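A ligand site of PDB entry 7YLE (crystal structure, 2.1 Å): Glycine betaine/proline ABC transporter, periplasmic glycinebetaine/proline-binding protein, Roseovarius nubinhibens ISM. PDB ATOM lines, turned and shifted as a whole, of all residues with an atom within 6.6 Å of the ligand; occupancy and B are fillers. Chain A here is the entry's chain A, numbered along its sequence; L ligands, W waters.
The backbone NH (N) of Ala 154 lies within hydrogen-bond range of an oxygen (O2) of the ligand.
The backbone NH (N) of Ala 153 lies within hydrogen-bond range of an oxygen (O1) of the ligand (2.7 Å).
S1 of the ligand sits close to NE1 of Trp 84 (3.7 Å).
OG1 of Thr 64 sits at hydrogen-bond distance from O1 of the ligand (2.6 Å).
The backbone NH (N) of Thr 64 is in hydrogen-bond range of the backbone carbonyl oxygen (O) of Gly 151 (3.4 Å).
OH of Tyr 242 is in hydrogen-bond range of O of Ala 154, 3.2 Å away.
OE1 of Glu 113 lies within hydrogen-bond range of OG of Ser 86.
The indole nitrogen (NE1) of Trp 84 is in hydrogen-bond range of the side-chain carboxylate (OE1) of Glu 82 (2.8 Å).
The side-chain carboxylate (OE2) of Glu 113 lies within hydrogen-bond range of the side-chain hydroxyl (OH) of Tyr 200.
The side-chain carboxylate (OE1) of Glu 82 sits at hydrogen-bond distance from the indole nitrogen (NE1) of Trp 35 (2.9 Å).
The backbone carbonyl oxygen of Ala 154 lies close to the side-chain hydroxyl of Ser 148 (3.1 Å).
O of Trp 202 is in hydrogen-bond range of OG1 of Thr 205, 2.9 Å away.
Trp 35 touches the ligand.
Glu 113 touches the ligand.
Trp 152 touches the ligand (CA to O1, 3.1 Å).
Tyr 200 touches the ligand (OH to C3, 3.6 Å).
CG of Trp 202 touches C4 of the ligand, at 3.4 Å.
Hydrophobic or aromatic side chains that line the ligand: Trp 35, Trp 84, Trp 152, Ala 153, Ala 154 and Trp 202.
Nine residues have an atom within 4 Å of the ligand: Trp 35, Thr 64, Trp 84, Glu 113, Trp 152, Ala 153, Ala 154, Tyr 200 and Trp 202.
The nearest printed residue that does not touch the ligand is Gly 151 (4.5 Å).
Water W1 lies within hydrogen-bond range of the side-chain carboxylate (OE2) of Glu 113 (2.6 Å), an oxygen (O2) of the ligand (2.8 Å), the side-chain hydroxyl (OG) of Ser 86 (3.1 Å) and the side-chain hydroxyl (OG) of Ser 87 (3.3 Å).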
ATOM      1  N   ASN A  34       1.076   4.370   9.971  1.00  0.00           N
ATOM      2  CA  ASN A  34       1.547   5.716   9.678  1.00  0.00           C
ATOM      3  C   ASN A  34       2.647   5.839   8.642  1.00  0.00           C
ATOM      4  O   ASN A  34       3.698   6.432   8.900  1.00  0.00           O
ATOM      5  CB  ASN A  34       1.934   6.459  10.975  1.00  0.00           C
ATOM      6  CG  ASN A  34       2.652   5.570  11.998  1.00  0.00           C
ATOM      7  OD1 ASN A  34       2.731   4.348  11.852  1.00  0.00           O
ATOM      8  ND2 ASN A  34       3.169   6.192  13.054  1.00  0.00           N
ATOM      9  N   TRP A  35       2.401   5.286   7.460  1.00  0.00           N
ATOM     10  CA  TRP A  35       3.237   5.517   6.295  1.00  0.00           C
ATOM     11  C   TRP A  35       2.414   5.340   5.015  1.00  0.00           C
ATOM     12  O   TRP A  35       1.285   4.855   5.072  1.00  0.00           O
ATOM     13  CB  TRP A  35       4.498   4.630   6.281  1.00  0.00           C
ATOM     14  CG  TRP A  35       4.271   3.137   6.428  1.00  0.00           C
ATOM     15  CD1 TRP A  35       4.164   2.223   5.415  1.00  0.00           C
ATOM     16  CD2 TRP A  35       4.159   2.387   7.653  1.00  0.00           C
ATOM     17  NE1 TRP A  35       3.981   0.968   5.941  1.00  0.00           N
ATOM     18  CE2 TRP A  35       3.982   1.044   7.312  1.00  0.00           C
ATOM     19  CE3 TRP A  35       4.199   2.745   9.009  1.00  0.00           C
ATOM     20  CZ2 TRP A  35       3.829   0.051   8.259  1.00  0.00           C
ATOM     21  CZ3 TRP A  35       4.057   1.756   9.944  1.00  0.00           C
ATOM     22  CH2 TRP A  35       3.875   0.413   9.574  1.00  0.00           C
ATOM     23  N   SER A  63       0.089   2.181  14.943  1.00  0.00           N
ATOM     24  CA  SER A  63       1.470   1.886  14.700  1.00  0.00           C
ATOM     25  C   SER A  63       1.685   0.434  15.102  1.00  0.00           C
ATOM     26  O   SER A  63       0.921  -0.094  15.903  1.00  0.00           O
ATOM     27  CB  SER A  63       2.354   2.805  15.546  1.00  0.00           C
ATOM     28  OG  SER A  63       3.511   3.123  14.821  1.00  0.00           O
ATOM     29  N   THR A  64       2.732  -0.188  14.572  1.00  0.00           N
ATOM     30  CA  THR A  64       2.944  -1.613  14.745  1.00  0.00           C
ATOM     31  C   THR A  64       2.886  -2.054  16.212  1.00  0.00           C
ATOM     32  O   THR A  64       2.120  -2.967  16.556  1.00  0.00           O
ATOM     33  CB  THR A  64       4.304  -2.018  14.162  1.00  0.00           C
ATOM     34  OG1 THR A  64       4.352  -1.613  12.791  1.00  0.00           O
ATOM     35  CG2 THR A  64       4.516  -3.513  14.271  1.00  0.00           C
ATOM     36  N   VAL A  65       3.683  -1.421  17.058  1.00  0.00           N
ATOM     37  CA  VAL A  65       3.789  -1.831  18.456  1.00  0.00           C
ATOM     38  C   VAL A  65       2.478  -1.674  19.253  1.00  0.00           C
ATOM     39  O   VAL A  65       2.014  -2.646  19.838  1.00  0.00           O
ATOM     40  CB  VAL A  65       4.962  -1.138  19.186  1.00  0.00           C
ATOM     41  CG1 VAL A  65       4.858  -1.345  20.697  1.00  0.00           C
ATOM     42  CG2 VAL A  65       6.288  -1.665  18.664  1.00  0.00           C
ATOM     43  N   GLU A  82      -0.828  -2.617   7.398  1.00  0.00           N
ATOM     44  CA  GLU A  82       0.219  -3.603   7.105  1.00  0.00           C
ATOM     45  C   GLU A  82       0.875  -4.062   8.385  1.00  0.00           C
ATOM     46  O   GLU A  82       1.168  -3.254   9.276  1.00  0.00           O
ATOM     47  CB  GLU A  82       1.332  -2.960   6.254  1.00  0.00           C
ATOM     48  CG  GLU A  82       0.915  -2.400   4.918  1.00  0.00           C
ATOM     49  CD  GLU A  82       2.043  -1.624   4.249  1.00  0.00           C
ATOM     50  OE1 GLU A  82       3.164  -1.579   4.832  1.00  0.00           O
ATOM     51  OE2 GLU A  82       1.819  -1.072   3.162  1.00  0.00           O
ATOM     52  N   TRP A  84       4.288  -5.589   9.468  1.00  0.00           N
ATOM     53  CA  TRP A  84       5.643  -5.971   9.096  1.00  0.00           C
ATOM     54  C   TRP A  84       6.154  -7.035  10.058  1.00  0.00           C
ATOM     55  O   TRP A  84       6.249  -6.778  11.262  1.00  0.00           O
ATOM     56  CB  TRP A  84       6.553  -4.727   9.093  1.00  0.00           C
ATOM     57  CG  TRP A  84       6.311  -3.929   7.847  1.00  0.00           C
ATOM     58  CD1 TRP A  84       5.162  -3.256   7.513  1.00  0.00           C
ATOM     59  CD2 TRP A  84       7.194  -3.762   6.742  1.00  0.00           C
ATOM     60  NE1 TRP A  84       5.295  -2.677   6.290  1.00  0.00           N
ATOM     61  CE2 TRP A  84       6.538  -2.963   5.778  1.00  0.00           C
ATOM     62  CE3 TRP A  84       8.501  -4.206   6.470  1.00  0.00           C
ATOM     63  CZ2 TRP A  84       7.118  -2.598   4.574  1.00  0.00           C
ATOM     64  CZ3 TRP A  84       9.090  -3.824   5.256  1.00  0.00           C
ATOM     65  CH2 TRP A  84       8.389  -3.039   4.326  1.00  0.00           C
ATOM     66  N   SER A  86       9.197  -8.600   9.997  1.00  0.00           N
ATOM     67  CA  SER A  86      10.658  -8.713  10.125  1.00  0.00           C
ATOM     68  C   SER A  86      11.102  -8.673  11.584  1.00  0.00           C
ATOM     69  O   SER A  86      12.080  -9.319  11.949  1.00  0.00           O
ATOM     70  CB  SER A  86      11.379  -7.592   9.384  1.00  0.00           C
ATOM     71  OG  SER A  86      10.836  -6.318   9.736  1.00  0.00           O
ATOM     72  N   SER A  87      10.410  -7.888  12.395  1.00  0.00           N
ATOM     73  CA  SER A  87      10.906  -7.580  13.732  1.00  0.00           C
ATOM     74  C   SER A  87       9.871  -7.848  14.779  1.00  0.00           C
ATOM     75  O   SER A  87       9.888  -7.246  15.839  1.00  0.00           O
ATOM     76  CB  SER A  87      11.371  -6.126  13.810  1.00  0.00           C
ATOM     77  OG  SER A  87      12.321  -5.873  12.782  1.00  0.00           O
ATOM     78  N   LEU A  88       8.964  -8.767  14.470  1.00  0.00           N
ATOM     79  CA  LEU A  88       7.986  -9.251  15.447  1.00  0.00           C
ATOM     80  C   LEU A  88       8.228 -10.747  15.719  1.00  0.00           C
ATOM     81  O   LEU A  88       7.454 -11.588  15.275  1.00  0.00           O
ATOM     82  CB  LEU A  88       6.568  -9.024  14.912  1.00  0.00           C
ATOM     83  CG  LEU A  88       6.110  -7.577  14.785  1.00  0.00           C
ATOM     84  CD1 LEU A  88       4.670  -7.504  14.288  1.00  0.00           C
ATOM     85  CD2 LEU A  88       6.248  -6.842  16.125  1.00  0.00           C
ATOM     86  N   GLU A 113      14.257  -3.578   4.978  1.00  0.00           N
ATOM     87  CA  GLU A 113      14.663  -2.499   5.866  1.00  0.00           C
ATOM     88  C   GLU A 113      16.171  -2.528   6.025  1.00  0.00           C
ATOM     89  O   GLU A 113      16.809  -3.559   5.837  1.00  0.00           O
ATOM     90  CB  GLU A 113      14.010  -2.694   7.225  1.00  0.00           C
ATOM     91  CG  GLU A 113      12.518  -2.536   7.197  1.00  0.00           C
ATOM     92  CD  GLU A 113      11.873  -3.273   8.344  1.00  0.00           C
ATOM     93  OE1 GLU A 113      11.822  -4.520   8.302  1.00  0.00           O
ATOM     94  OE2 GLU A 113      11.416  -2.603   9.278  1.00  0.00           O
ATOM     95  N   SER A 148      14.335   5.185  13.343  1.00  0.00           N
ATOM     96  CA  SER A 148      12.903   5.039  13.128  1.00  0.00           C
ATOM     97  C   SER A 148      12.117   5.535  14.347  1.00  0.00           C
ATOM     98  O   SER A 148      12.649   5.536  15.465  1.00  0.00           O
ATOM     99  CB  SER A 148      12.582   3.566  12.879  1.00  0.00           C
ATOM    100  OG  SER A 148      13.190   2.759  13.884  1.00  0.00           O
ATOM    101  N   GLY A 151       7.018   3.564  18.256  1.00  0.00           N
ATOM    102  CA  GLY A 151       5.797   2.899  17.838  1.00  0.00           C
ATOM    103  C   GLY A 151       6.048   1.870  16.752  1.00  0.00           C
ATOM    104  O   GLY A 151       5.219   0.988  16.525  1.00  0.00           O
ATOM    105  N   TRP A 152       7.191   1.991  16.077  1.00  0.00           N
ATOM    106  CA  TRP A 152       7.572   0.998  15.083  1.00  0.00           C
ATOM    107  C   TRP A 152       8.411  -0.060  15.764  1.00  0.00           C
ATOM    108  O   TRP A 152       9.184   0.234  16.679  1.00  0.00           O
ATOM    109  CB  TRP A 152       8.367   1.633  13.945  1.00  0.00           C
ATOM    110  CG  TRP A 152       7.534   2.593  13.089  1.00  0.00           C
ATOM    111  CD1 TRP A 152       6.283   3.066  13.359  1.00  0.00           C
ATOM    112  CD2 TRP A 152       7.929   3.161  11.831  1.00  0.00           C
ATOM    113  NE1 TRP A 152       5.877   3.911  12.349  1.00  0.00           N
ATOM    114  CE2 TRP A 152       6.856   3.984  11.402  1.00  0.00           C
ATOM    115  CE3 TRP A 152       9.076   3.071  11.033  1.00  0.00           C
ATOM    116  CZ2 TRP A 152       6.897   4.714  10.192  1.00  0.00           C
ATOM    117  CZ3 TRP A 152       9.107   3.791   9.828  1.00  0.00           C
ATOM    118  CH2 TRP A 152       8.030   4.603   9.434  1.00  0.00           C
ATOM    119  N   ALA A 153       8.264  -1.309  15.315  1.00  0.00           N
ATOM    120  CA  ALA A 153       9.098  -2.388  15.835  1.00  0.00           C
ATOM    121  C   ALA A 153      10.551  -2.088  15.491  1.00  0.00           C
ATOM    122  O   ALA A 153      11.467  -2.406  16.239  1.00  0.00           O
ATOM    123  CB  ALA A 153       8.676  -3.714  15.229  1.00  0.00           C
ATOM    124  N   ALA A 154      10.768  -1.440  14.340  1.00  0.00           N
ATOM    125  CA  ALA A 154      12.097  -1.008  13.930  1.00  0.00           C
ATOM    126  C   ALA A 154      12.810  -0.107  14.969  1.00  0.00           C
ATOM    127  O   ALA A 154      14.033  -0.063  14.992  1.00  0.00           O
ATOM    128  CB  ALA A 154      12.023  -0.300  12.583  1.00  0.00           C
ATOM    129  N   ALA A 155      12.067   0.620  15.793  1.00  0.00           N
ATOM    130  CA  ALA A 155      12.712   1.506  16.775  1.00  0.00           C
ATOM    131  C   ALA A 155      13.422   0.684  17.862  1.00  0.00           C
ATOM    132  O   ALA A 155      14.463   1.092  18.395  1.00  0.00           O
ATOM    133  CB  ALA A 155      11.701   2.468  17.389  1.00  0.00           C
ATOM    134  N   TYR A 200      17.801   4.780   9.311  1.00  0.00           N
ATOM    135  CA  TYR A 200      16.862   3.715   8.974  1.00  0.00           C
ATOM    136  C   TYR A 200      15.983   4.152   7.841  1.00  0.00           C
ATOM    137  O   TYR A 200      15.477   5.280   7.824  1.00  0.00           O
ATOM    138  CB  TYR A 200      15.967   3.386  10.184  1.00  0.00           C
ATOM    139  CG  TYR A 200      14.782   2.478   9.834  1.00  0.00           C
ATOM    140  CD1 TYR A 200      13.582   3.007   9.354  1.00  0.00           C
ATOM    141  CD2 TYR A 200      14.854   1.096  10.024  1.00  0.00           C
ATOM    142  CE1 TYR A 200      12.492   2.187   9.051  1.00  0.00           C
ATOM    143  CE2 TYR A 200      13.767   0.262   9.720  1.00  0.00           C
ATOM    144  CZ  TYR A 200      12.602   0.822   9.242  1.00  0.00           C
ATOM    145  OH  TYR A 200      11.534   0.000   8.935  1.00  0.00           O
ATOM    146  N   TYR A 201      15.799   3.260   6.874  1.00  0.00           N
ATOM    147  CA  TYR A 201      14.699   3.380   5.929  1.00  0.00           C
ATOM    148  C   TYR A 201      14.410   2.023   5.322  1.00  0.00           C
ATOM    149  O   TYR A 201      14.984   1.014   5.745  1.00  0.00           O
ATOM    150  CB  TYR A 201      14.951   4.485   4.874  1.00  0.00           C
ATOM    151  CG  TYR A 201      13.670   5.231   4.589  1.00  0.00           C
ATOM    152  CD1 TYR A 201      13.114   6.064   5.551  1.00  0.00           C
ATOM    153  CD2 TYR A 201      12.950   5.024   3.403  1.00  0.00           C
ATOM    154  CE1 TYR A 201      11.896   6.712   5.332  1.00  0.00           C
ATOM    155  CE2 TYR A 201      11.734   5.674   3.171  1.00  0.00           C
ATOM    156  CZ  TYR A 201      11.224   6.525   4.149  1.00  0.00           C
ATOM    157  OH  TYR A 201      10.023   7.169   3.954  1.00  0.00           O
ATOM    158  N   TRP A 202      13.513   1.985   4.347  1.00  0.00           N
ATOM    159  CA  TRP A 202      13.119   0.727   3.724  1.00  0.00           C
ATOM    160  C   TRP A 202      12.820   0.895   2.232  1.00  0.00           C
ATOM    161  O   TRP A 202      12.569   2.006   1.745  1.00  0.00           O
ATOM    162  CB  TRP A 202      11.941   0.087   4.478  1.00  0.00           C
ATOM    163  CG  TRP A 202      10.567   0.736   4.304  1.00  0.00           C
ATOM    164  CD1 TRP A 202       9.533   0.287   3.522  1.00  0.00           C
ATOM    165  CD2 TRP A 202      10.068   1.916   4.972  1.00  0.00           C
ATOM    166  NE1 TRP A 202       8.434   1.108   3.645  1.00  0.00           N
ATOM    167  CE2 TRP A 202       8.744   2.118   4.523  1.00  0.00           C
ATOM    168  CE3 TRP A 202      10.626   2.827   5.883  1.00  0.00           C
ATOM    169  CZ2 TRP A 202       7.961   3.193   4.957  1.00  0.00           C
ATOM    170  CZ3 TRP A 202       9.856   3.899   6.312  1.00  0.00           C
ATOM    171  CH2 TRP A 202       8.531   4.080   5.840  1.00  0.00           C
ATOM    172  N   THR A 205      10.441   2.216  -1.728  1.00  0.00           N
ATOM    173  CA  THR A 205       9.564   3.301  -1.259  1.00  0.00           C
ATOM    174  C   THR A 205       9.635   4.479  -2.230  1.00  0.00           C
ATOM    175  O   THR A 205      10.539   4.547  -3.054  1.00  0.00           O
ATOM    176  CB  THR A 205       9.965   3.831   0.128  1.00  0.00           C
ATOM    177  OG1 THR A 205      11.363   4.147   0.144  1.00  0.00           O
ATOM    178  CG2 THR A 205       9.654   2.812   1.210  1.00  0.00           C
ATOM    179  N   TYR A 242      18.664  -6.394   9.198  1.00  0.00           N
ATOM    180  CA  TYR A 242      17.284  -6.838   9.200  1.00  0.00           C
ATOM    181  C   TYR A 242      17.131  -7.946   8.181  1.00  0.00           C
ATOM    182  O   TYR A 242      17.811  -7.918   7.162  1.00  0.00           O
ATOM    183  CB  TYR A 242      16.359  -5.698   8.744  1.00  0.00           C
ATOM    184  CG  TYR A 242      16.113  -4.567   9.732  1.00  0.00           C
ATOM    185  CD1 TYR A 242      17.075  -3.600   9.969  1.00  0.00           C
ATOM    186  CD2 TYR A 242      14.906  -4.478  10.410  1.00  0.00           C
ATOM    187  CE1 TYR A 242      16.839  -2.564  10.863  1.00  0.00           C
ATOM    188  CE2 TYR A 242      14.661  -3.452  11.309  1.00  0.00           C
ATOM    189  CZ  TYR A 242      15.632  -2.496  11.518  1.00  0.00           C
ATOM    190  OH  TYR A 242      15.380  -1.462  12.394  1.00  0.00           O
ATOM    191  N   VAL A 247       5.164  -8.999   4.837  1.00  0.00           N
ATOM    192  CA  VAL A 247       4.271  -7.938   5.265  1.00  0.00           C
ATOM    193  C   VAL A 247       2.861  -8.421   5.042  1.00  0.00           C
ATOM    194  O   VAL A 247       2.448  -8.639   3.909  1.00  0.00           O
ATOM    195  CB  VAL A 247       4.511  -6.673   4.440  1.00  0.00           C
ATOM    196  CG1 VAL A 247       3.531  -5.569   4.879  1.00  0.00           C
ATOM    197  CG2 VAL A 247       5.985  -6.220   4.592  1.00  0.00           C
HETATM  198  S1  LIG L   1       7.661  -0.424   8.043  1.00  0.00           S
HETATM  199  C1  LIG L   1       7.668  -1.195  12.013  1.00  0.00           C
HETATM  200  O1  LIG L   1       6.892  -1.232  12.999  1.00  0.00           O
HETATM  201  C2  LIG L   1       7.125  -0.979  10.627  1.00  0.00           C
HETATM  202  O2  LIG L   1       8.907  -1.346  12.192  1.00  0.00           O
HETATM  203  C3  LIG L   1       8.182  -1.172   9.566  1.00  0.00           C
HETATM  204  C4  LIG L   1       8.678  -0.628   6.728  1.00  0.00           C
HETATM  205  C5  LIG L   1       6.974   1.087   7.933  1.00  0.00           C
HETATM  206  O   HOH W   1      10.292  -3.676  11.346  1.00  0.00           O
